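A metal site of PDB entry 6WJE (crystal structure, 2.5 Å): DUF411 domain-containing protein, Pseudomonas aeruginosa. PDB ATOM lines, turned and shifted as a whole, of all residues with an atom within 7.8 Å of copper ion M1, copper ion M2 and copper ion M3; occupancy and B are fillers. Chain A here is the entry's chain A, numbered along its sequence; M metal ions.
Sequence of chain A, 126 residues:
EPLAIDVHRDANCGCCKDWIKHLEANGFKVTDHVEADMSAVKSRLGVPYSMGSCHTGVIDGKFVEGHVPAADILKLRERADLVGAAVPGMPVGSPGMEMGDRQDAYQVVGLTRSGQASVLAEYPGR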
ATOM      1  N   VAL A   7      -0.704   7.127 -14.928  1.00  0.00           N
ATOM      2  CA  VAL A   7      -0.947   8.486 -14.456  1.00  0.00           C
ATOM      3  C   VAL A   7      -1.076   8.472 -12.934  1.00  0.00           C
ATOM      4  O   VAL A   7      -1.759   7.598 -12.389  1.00  0.00           O
ATOM      5  CB  VAL A   7      -2.193   9.104 -15.121  1.00  0.00           C
ATOM      6  CG1 VAL A   7      -2.459  10.517 -14.610  1.00  0.00           C
ATOM      7  CG2 VAL A   7      -1.957   9.148 -16.617  1.00  0.00           C
ATOM      8  N   HIS A   8      -0.368   9.380 -12.260  1.00  0.00           N
ATOM      9  CA  HIS A   8      -0.553   9.632 -10.838  1.00  0.00           C
ATOM     10  C   HIS A   8      -1.165  11.019 -10.698  1.00  0.00           C
ATOM     11  O   HIS A   8      -0.746  11.966 -11.384  1.00  0.00           O
ATOM     12  CB  HIS A   8       0.774   9.576  -9.998  1.00  0.00           C
ATOM     13  CG  HIS A   8       1.456   8.210  -9.959  1.00  0.00           C
ATOM     14  ND1 HIS A   8       1.711   7.493  -8.788  1.00  0.00           N
ATOM     15  CD2 HIS A   8       1.959   7.467 -10.960  1.00  0.00           C
ATOM     16  CE1 HIS A   8       2.313   6.361  -9.101  1.00  0.00           C
ATOM     17  NE2 HIS A   8       2.482   6.332 -10.409  1.00  0.00           N
ATOM     18  N   ARG A   9      -2.152  11.162  -9.822  1.00  0.00           N
ATOM     19  CA  ARG A   9      -2.802  12.445  -9.611  1.00  0.00           C
ATOM     20  C   ARG A   9      -3.502  12.425  -8.270  1.00  0.00           C
ATOM     21  O   ARG A   9      -3.729  11.373  -7.672  1.00  0.00           O
ATOM     22  CB  ARG A   9      -3.790  12.775 -10.729  1.00  0.00           C
ATOM     23  CG  ARG A   9      -4.727  11.658 -11.049  1.00  0.00           C
ATOM     24  CD  ARG A   9      -6.010  11.908 -10.419  1.00  0.00           C
ATOM     25  NE  ARG A   9      -6.968  10.853 -10.696  1.00  0.00           N
ATOM     26  CZ  ARG A   9      -8.133  10.733 -10.043  1.00  0.00           C
ATOM     27  NH1 ARG A   9      -8.447  11.611  -9.087  1.00  0.00           N
ATOM     28  NH2 ARG A   9      -8.967   9.753 -10.350  1.00  0.00           N
ATOM     29  N   ASP A  10      -3.856  13.626  -7.810  1.00  0.00           N
ATOM     30  CA  ASP A  10      -4.597  13.802  -6.570  1.00  0.00           C
ATOM     31  C   ASP A  10      -6.070  13.405  -6.710  1.00  0.00           C
ATOM     32  O   ASP A  10      -6.671  13.478  -7.793  1.00  0.00           O
ATOM     33  CB  ASP A  10      -4.461  15.268  -6.136  1.00  0.00           C
ATOM     34  CG  ASP A  10      -5.143  15.572  -4.819  1.00  0.00           C
ATOM     35  OD1 ASP A  10      -4.537  15.304  -3.746  1.00  0.00           O
ATOM     36  OD2 ASP A  10      -6.280  16.103  -4.867  1.00  0.00           O
ATOM     37  N   CYS A  13      -8.551  16.122  -8.215  1.00  0.00           N
ATOM     38  CA  CYS A  13      -8.117  16.828  -9.440  1.00  0.00           C
ATOM     39  C   CYS A  13      -9.048  16.378 -10.542  1.00  0.00           C
ATOM     40  O   CYS A  13      -8.814  15.368 -11.206  1.00  0.00           O
ATOM     41  CB  CYS A  13      -6.649  16.594  -9.804  1.00  0.00           C
ATOM     42  SG  CYS A  13      -6.064  17.601 -11.314  1.00  0.00           S
ATOM     43  N   GLY A  14     -10.093  17.161 -10.742  1.00  0.00           N
ATOM     44  CA  GLY A  14     -11.073  16.854 -11.737  1.00  0.00           C
ATOM     45  C   GLY A  14     -10.616  17.105 -13.161  1.00  0.00           C
ATOM     46  O   GLY A  14     -10.954  16.316 -14.035  1.00  0.00           O
ATOM     47  N   CYS A  15      -9.946  18.230 -13.431  1.00  0.00           N
ATOM     48  CA  CYS A  15      -9.326  18.361 -14.738  1.00  0.00           C
ATOM     49  C   CYS A  15      -8.475  17.147 -15.072  1.00  0.00           C
ATOM     50  O   CYS A  15      -8.585  16.605 -16.180  1.00  0.00           O
ATOM     51  CB  CYS A  15      -8.551  19.690 -14.860  1.00  0.00           C
ATOM     52  SG  CYS A  15      -7.212  19.921 -13.648  1.00  0.00           S
ATOM     53  N   CYS A  16      -7.666  16.686 -14.121  1.00  0.00           N
ATOM     54  CA  CYS A  16      -6.839  15.494 -14.354  1.00  0.00           C
ATOM     55  C   CYS A  16      -7.679  14.290 -14.774  1.00  0.00           C
ATOM     56  O   CYS A  16      -7.271  13.526 -15.662  1.00  0.00           O
ATOM     57  CB  CYS A  16      -6.017  15.124 -13.109  1.00  0.00           C
ATOM     58  SG  CYS A  16      -4.890  16.434 -12.535  1.00  0.00           S
ATOM     59  N   LYS A  17      -8.870  14.111 -14.174  1.00  0.00           N
ATOM     60  CA  LYS A  17      -9.722  13.014 -14.597  1.00  0.00           C
ATOM     61  C   LYS A  17     -10.239  13.225 -16.014  1.00  0.00           C
ATOM     62  O   LYS A  17     -10.349  12.269 -16.794  1.00  0.00           O
ATOM     63  CB  LYS A  17     -10.902  12.842 -13.656  1.00  0.00           C
ATOM     64  CG  LYS A  17     -10.629  12.386 -12.239  1.00  0.00           C
ATOM     65  CD  LYS A  17     -11.958  12.458 -11.432  1.00  0.00           C
ATOM     66  CE  LYS A  17     -11.796  12.273  -9.921  1.00  0.00           C
ATOM     67  N   ASP A  18     -10.530  14.486 -16.344  1.00  0.00           N
ATOM     68  CA  ASP A  18     -11.042  14.842 -17.710  1.00  0.00           C
ATOM     69  C   ASP A  18      -9.980  14.460 -18.753  1.00  0.00           C
ATOM     70  O   ASP A  18     -10.358  13.865 -19.775  1.00  0.00           O
ATOM     71  CB  ASP A  18     -11.405  16.328 -17.778  1.00  0.00           C
ATOM     72  CG  ASP A  18     -12.142  16.706 -19.053  1.00  0.00           C
ATOM     73  OD1 ASP A  18     -12.784  15.812 -19.653  1.00  0.00           O
ATOM     74  OD2 ASP A  18     -12.063  17.882 -19.451  1.00  0.00           O
ATOM     75  N   TRP A  19      -8.722  14.804 -18.483  1.00  0.00           N
ATOM     76  CA  TRP A  19      -7.605  14.506 -19.383  1.00  0.00           C
ATOM     77  C   TRP A  19      -7.468  13.009 -19.621  1.00  0.00           C
ATOM     78  O   TRP A  19      -7.285  12.579 -20.763  1.00  0.00           O
ATOM     79  CB  TRP A  19      -6.306  15.080 -18.804  1.00  0.00           C
ATOM     80  CG  TRP A  19      -5.040  14.860 -19.620  1.00  0.00           C
ATOM     81  CD1 TRP A  19      -4.686  15.523 -20.776  1.00  0.00           C
ATOM     82  CD2 TRP A  19      -3.962  13.959 -19.345  1.00  0.00           C
ATOM     83  NE1 TRP A  19      -3.458  15.094 -21.216  1.00  0.00           N
ATOM     84  CE2 TRP A  19      -3.000  14.121 -20.357  1.00  0.00           C
ATOM     85  CE3 TRP A  19      -3.722  13.041 -18.322  1.00  0.00           C
ATOM     86  CZ2 TRP A  19      -1.804  13.399 -20.384  1.00  0.00           C
ATOM     87  CZ3 TRP A  19      -2.539  12.310 -18.343  1.00  0.00           C
ATOM     88  CH2 TRP A  19      -1.595  12.493 -19.378  1.00  0.00           C
ATOM     89  N   LYS A  42       7.081  13.620  -9.141  1.00  0.00           N
ATOM     90  CA  LYS A  42       7.789  14.510 -10.060  1.00  0.00           C
ATOM     91  C   LYS A  42       9.287  14.472  -9.795  1.00  0.00           C
ATOM     92  O   LYS A  42      10.107  14.573 -10.736  1.00  0.00           O
ATOM     93  CB  LYS A  42       7.257  15.932  -9.925  1.00  0.00           C
ATOM     94  CG  LYS A  42       5.869  16.143 -10.472  1.00  0.00           C
ATOM     95  CD  LYS A  42       5.301  17.446  -9.971  1.00  0.00           C
ATOM     96  CE  LYS A  42       3.771  17.425  -9.917  1.00  0.00           C
ATOM     97  NZ  LYS A  42       3.149  17.060 -11.235  1.00  0.00           N
ATOM     98  N   SER A  53       3.010  20.750 -13.042  1.00  0.00           N
ATOM     99  CA  SER A  53       1.601  20.826 -13.377  1.00  0.00           C
ATOM    100  C   SER A  53       0.802  19.975 -12.393  1.00  0.00           C
ATOM    101  O   SER A  53       1.300  19.586 -11.337  1.00  0.00           O
ATOM    102  CB  SER A  53       1.367  20.372 -14.822  1.00  0.00           C
ATOM    103  OG  SER A  53       0.174  20.941 -15.299  1.00  0.00           O
ATOM    104  N   CYS A  54      -0.474  19.752 -12.714  1.00  0.00           N
ATOM    105  CA  CYS A  54      -1.438  19.075 -11.853  1.00  0.00           C
ATOM    106  C   CYS A  54      -1.271  17.556 -11.812  1.00  0.00           C
ATOM    107  O   CYS A  54      -1.830  16.933 -10.914  1.00  0.00           O
ATOM    108  CB  CYS A  54      -2.867  19.428 -12.249  1.00  0.00           C
ATOM    109  SG  CYS A  54      -3.194  19.355 -13.981  1.00  0.00           S
ATOM    110  N   HIS A  55      -0.655  16.931 -12.820  1.00  0.00           N
ATOM    111  CA  HIS A  55      -0.602  15.476 -12.812  1.00  0.00           C
ATOM    112  C   HIS A  55       0.685  15.091 -13.522  1.00  0.00           C
ATOM    113  O   HIS A  55       1.209  15.852 -14.337  1.00  0.00           O
ATOM    114  CB  HIS A  55      -1.818  14.831 -13.484  1.00  0.00           C
ATOM    115  CG  HIS A  55      -1.906  15.094 -14.955  1.00  0.00           C
ATOM    116  ND1 HIS A  55      -2.833  15.953 -15.522  1.00  0.00           N
ATOM    117  CD2 HIS A  55      -1.225  14.563 -15.995  1.00  0.00           C
ATOM    118  CE1 HIS A  55      -2.670  15.990 -16.830  1.00  0.00           C
ATOM    119  NE2 HIS A  55      -1.709  15.141 -17.145  1.00  0.00           N
ATOM    120  N   THR A  56       1.142  13.848 -13.273  1.00  0.00           N
ATOM    121  CA  THR A  56       2.357  13.317 -13.888  1.00  0.00           C
ATOM    122  C   THR A  56       2.118  11.919 -14.423  1.00  0.00           C
ATOM    123  O   THR A  56       1.805  10.999 -13.656  1.00  0.00           O
ATOM    124  CB  THR A  56       3.522  13.264 -12.888  1.00  0.00           C
ATOM    125  OG1 THR A  56       3.687  14.554 -12.285  1.00  0.00           O
ATOM    126  CG2 THR A  56       4.813  12.887 -13.593  1.00  0.00           C
ATOM    127  N   GLU A  65       4.048  15.547 -18.327  1.00  0.00           N
ATOM    128  CA  GLU A  65       3.664  16.466 -17.260  1.00  0.00           C
ATOM    129  C   GLU A  65       2.552  17.393 -17.745  1.00  0.00           C
ATOM    130  O   GLU A  65       2.778  18.239 -18.617  1.00  0.00           O
ATOM    131  CB  GLU A  65       4.846  17.292 -16.787  1.00  0.00           C
ATOM    132  CG  GLU A  65       4.458  18.173 -15.615  1.00  0.00           C
ATOM    133  CD  GLU A  65       4.400  17.410 -14.276  1.00  0.00           C
ATOM    134  OE1 GLU A  65       4.896  16.270 -14.199  1.00  0.00           O
ATOM    135  OE2 GLU A  65       3.831  17.952 -13.299  1.00  0.00           O
ATOM    136  N   GLY A  66       1.377  17.286 -17.109  1.00  0.00           N
ATOM    137  CA  GLY A  66       0.260  18.149 -17.391  1.00  0.00           C
ATOM    138  C   GLY A  66      -0.555  17.720 -18.606  1.00  0.00           C
ATOM    139  O   GLY A  66      -0.484  16.590 -19.084  1.00  0.00           O
ATOM    140  N   HIS A  67      -1.337  18.677 -19.101  1.00  0.00           N
ATOM    141  CA  HIS A  67      -2.391  18.434 -20.096  1.00  0.00           C
ATOM    142  C   HIS A  67      -1.798  18.443 -21.499  1.00  0.00           C
ATOM    143  O   HIS A  67      -2.105  19.308 -22.324  1.00  0.00           O
ATOM    144  CB  HIS A  67      -3.486  19.485 -19.968  1.00  0.00           C
ATOM    145  CG  HIS A  67      -4.285  19.352 -18.717  1.00  0.00           C
ATOM    146  ND1 HIS A  67      -5.475  18.662 -18.671  1.00  0.00           N
ATOM    147  CD2 HIS A  67      -3.997  19.702 -17.439  1.00  0.00           C
ATOM    148  CE1 HIS A  67      -5.933  18.666 -17.431  1.00  0.00           C
ATOM    149  NE2 HIS A  67      -5.048  19.284 -16.659  1.00  0.00           N
ATOM    150  N   GLY A  89       1.772  24.290 -15.616  1.00  0.00           N
ATOM    151  CA  GLY A  89       0.568  24.981 -15.155  1.00  0.00           C
ATOM    152  C   GLY A  89      -0.698  24.314 -15.658  1.00  0.00           C
ATOM    153  O   GLY A  89      -0.734  23.094 -15.900  1.00  0.00           O
ATOM    154  N   MET A  90      -1.742  25.110 -15.885  1.00  0.00           N
ATOM    155  CA  MET A  90      -3.058  24.601 -16.307  1.00  0.00           C
ATOM    156  C   MET A  90      -3.720  25.551 -17.301  1.00  0.00           C
ATOM    157  O   MET A  90      -4.733  26.173 -16.999  1.00  0.00           O
ATOM    158  CB  MET A  90      -3.957  24.353 -15.093  1.00  0.00           C
ATOM    159  CG  MET A  90      -3.611  23.079 -14.331  1.00  0.00           C
ATOM    160  SD  MET A  90      -4.741  22.610 -13.004  1.00  0.00           S
ATOM    161  CE  MET A  90      -5.358  24.230 -12.564  1.00  0.00           C
ATOM    162  N   PRO A  91      -3.197  25.642 -18.526  1.00  0.00           N
ATOM    163  CA  PRO A  91      -3.778  26.569 -19.509  1.00  0.00           C
ATOM    164  C   PRO A  91      -5.190  26.162 -19.912  1.00  0.00           C
ATOM    165  O   PRO A  91      -5.460  24.990 -20.151  1.00  0.00           O
ATOM    166  CB  PRO A  91      -2.803  26.478 -20.695  1.00  0.00           C
ATOM    167  CG  PRO A  91      -2.098  25.185 -20.530  1.00  0.00           C
ATOM    168  CD  PRO A  91      -2.014  24.929 -19.043  1.00  0.00           C
ATOM    169  N   VAL A  92      -6.112  27.130 -19.895  1.00  0.00           N
ATOM    170  CA  VAL A  92      -7.487  26.847 -20.313  1.00  0.00           C
ATOM    171  C   VAL A  92      -7.519  26.503 -21.792  1.00  0.00           C
ATOM    172  O   VAL A  92      -6.936  27.210 -22.635  1.00  0.00           O
ATOM    173  CB  VAL A  92      -8.391  28.035 -19.970  1.00  0.00           C
ATOM    174  CG1 VAL A  92      -9.884  27.744 -20.201  1.00  0.00           C
ATOM    175  CG2 VAL A  92      -8.189  28.382 -18.524  1.00  0.00           C
ATOM    176  N   SER A  94      -6.501  23.543 -22.975  1.00  0.00           N
ATOM    177  CA  SER A  94      -5.759  22.327 -23.197  1.00  0.00           C
ATOM    178  C   SER A  94      -6.701  21.175 -22.860  1.00  0.00           C
ATOM    179  O   SER A  94      -7.693  21.368 -22.150  1.00  0.00           O
ATOM    180  CB  SER A  94      -4.486  22.278 -22.364  1.00  0.00           C
ATOM    181  OG  SER A  94      -4.756  22.230 -20.971  1.00  0.00           O
ATOM    182  N   PRO A  95      -6.436  19.975 -23.375  1.00  0.00           N
ATOM    183  CA  PRO A  95      -7.392  18.871 -23.193  1.00  0.00           C
ATOM    184  C   PRO A  95      -7.574  18.515 -21.723  1.00  0.00           C
ATOM    185  O   PRO A  95      -6.603  18.295 -20.998  1.00  0.00           O
ATOM    186  CB  PRO A  95      -6.745  17.720 -23.977  1.00  0.00           C
ATOM    187  CG  PRO A  95      -5.743  18.342 -24.866  1.00  0.00           C
ATOM    188  CD  PRO A  95      -5.286  19.593 -24.217  1.00  0.00           C
ATOM    189  N   GLY A  96      -8.828  18.429 -21.289  1.00  0.00           N
ATOM    190  CA  GLY A  96      -9.143  18.240 -19.890  1.00  0.00           C
ATOM    191  C   GLY A  96      -9.230  19.517 -19.101  1.00  0.00           C
ATOM    192  O   GLY A  96      -9.651  19.485 -17.925  1.00  0.00           O
ATOM    193  N   MET A  97      -8.849  20.647 -19.693  1.00  0.00           N
ATOM    194  CA  MET A  97      -8.970  21.952 -19.069  1.00  0.00           C
ATOM    195  C   MET A  97      -9.879  22.877 -19.883  1.00  0.00           C
ATOM    196  O   MET A  97      -9.847  24.105 -19.727  1.00  0.00           O
ATOM    197  CB  MET A  97      -7.571  22.579 -18.891  1.00  0.00           C
ATOM    198  CG  MET A  97      -6.894  22.272 -17.524  1.00  0.00           C
ATOM    199  SD  MET A  97      -7.832  22.887 -16.092  1.00  0.00           S
ATOM    200  CE  MET A  97      -7.762  24.663 -16.250  1.00  0.00           C
ATOM    201  N   GLU A  98     -10.719  22.306 -20.744  1.00  0.00           N
ATOM    202  CA  GLU A  98     -11.502  23.094 -21.684  1.00  0.00           C
ATOM    203  C   GLU A  98     -12.677  23.777 -20.969  1.00  0.00           C
ATOM    204  O   GLU A  98     -13.405  23.155 -20.194  1.00  0.00           O
ATOM    205  CB  GLU A  98     -11.955  22.178 -22.847  1.00  0.00           C
ATOM    206  CG  GLU A  98     -13.215  21.279 -22.683  1.00  0.00           C
ATOM    207  CD  GLU A  98     -13.023  19.814 -22.164  1.00  0.00           C
ATOM    208  OE1 GLU A  98     -11.912  19.332 -21.821  1.00  0.00           O
ATOM    209  OE2 GLU A  98     -14.055  19.084 -22.128  1.00  0.00           O
ATOM    210  N   MET A  99     -12.831  25.068 -21.184  1.00  0.00           N
ATOM    211  CA  MET A  99     -13.825  25.827 -20.442  1.00  0.00           C
ATOM    212  C   MET A  99     -14.502  26.834 -21.361  1.00  0.00           C
ATOM    213  O   MET A  99     -14.631  28.021 -21.056  1.00  0.00           O
ATOM    214  CB  MET A  99     -13.182  26.490 -19.241  1.00  0.00           C
ATOM    215  CG  MET A  99     -13.355  25.712 -17.998  1.00  0.00           C
ATOM    216  SD  MET A  99     -12.170  26.347 -16.837  1.00  0.00           S
ATOM    217  CE  MET A  99     -11.263  24.849 -16.575  1.00  0.00           C
HETATM  218 CU    CU M   1      -6.892  22.249 -14.053  1.00  0.00          CU
HETATM  219 CU    CU M   2      -5.246  19.508 -14.633  1.00  0.00          CU
HETATM  220 CU    CU M   3      -3.651  17.291 -14.102  1.00  0.00          CU
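A ring nitrogen (ND1) of His 67 is in hydrogen-bond range of the backbone carbonyl oxygen of Pro 95 (2.6 Å).
SG of Cys 16 forms a disulfide with SG of Cys 13 (2.1 Å).
SG of Cys 13 lies close to SG of Cys 15, 3.5 Å away.
A ring nitrogen (NE2) of His 55 sits at hydrogen-bond distance from the backbone carbonyl oxygen of Gly 66 (2.7 Å).
Of the 29 residues printed, 3 come within 4 Å of copper ion M1.
The nearest printed residue that does not touch copper ion M1 is His 67 (4.4 Å).
Cys 13 touches copper ion M2 (SG to CU, 3.9 Å).
Along chain A the residues within 4 Å of copper ion M2 span positions 13 to 90.
Merely in contact with copper ion M3: Cys 13.
Within 4 Å of copper ion M3: Cys 13, Cys 16, Cys 54, His 55 and His 67.
The nearest printed residue that does not touch copper ion M3 is Cys 15 (4.5 Å).
Copper ion M1 is bound by the side-chain sulfur (SD) of Met 97, 2.3 Å away.
Copper ion M1 is bound by SG of Cys 15 (2.4 Å).
Copper ion M1 is bound by the side-chain sulfur (SD) of Met 90, at 2.4 Å.
A ring nitrogen (NE2) of His 67 binds copper ion M2, at 2.0 Å.
Copper ion M2 is bound by SG of Cys 54.
Copper ion M2 is bound by the side-chain sulfur (SG) of Cys 15 (2.2 Å).
Copper ion M3 is bound by ND1 of His 55 (2.1 Å), SG of Cys 54 (2.1 Å) and SG of Cys 16 (2.2 Å).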
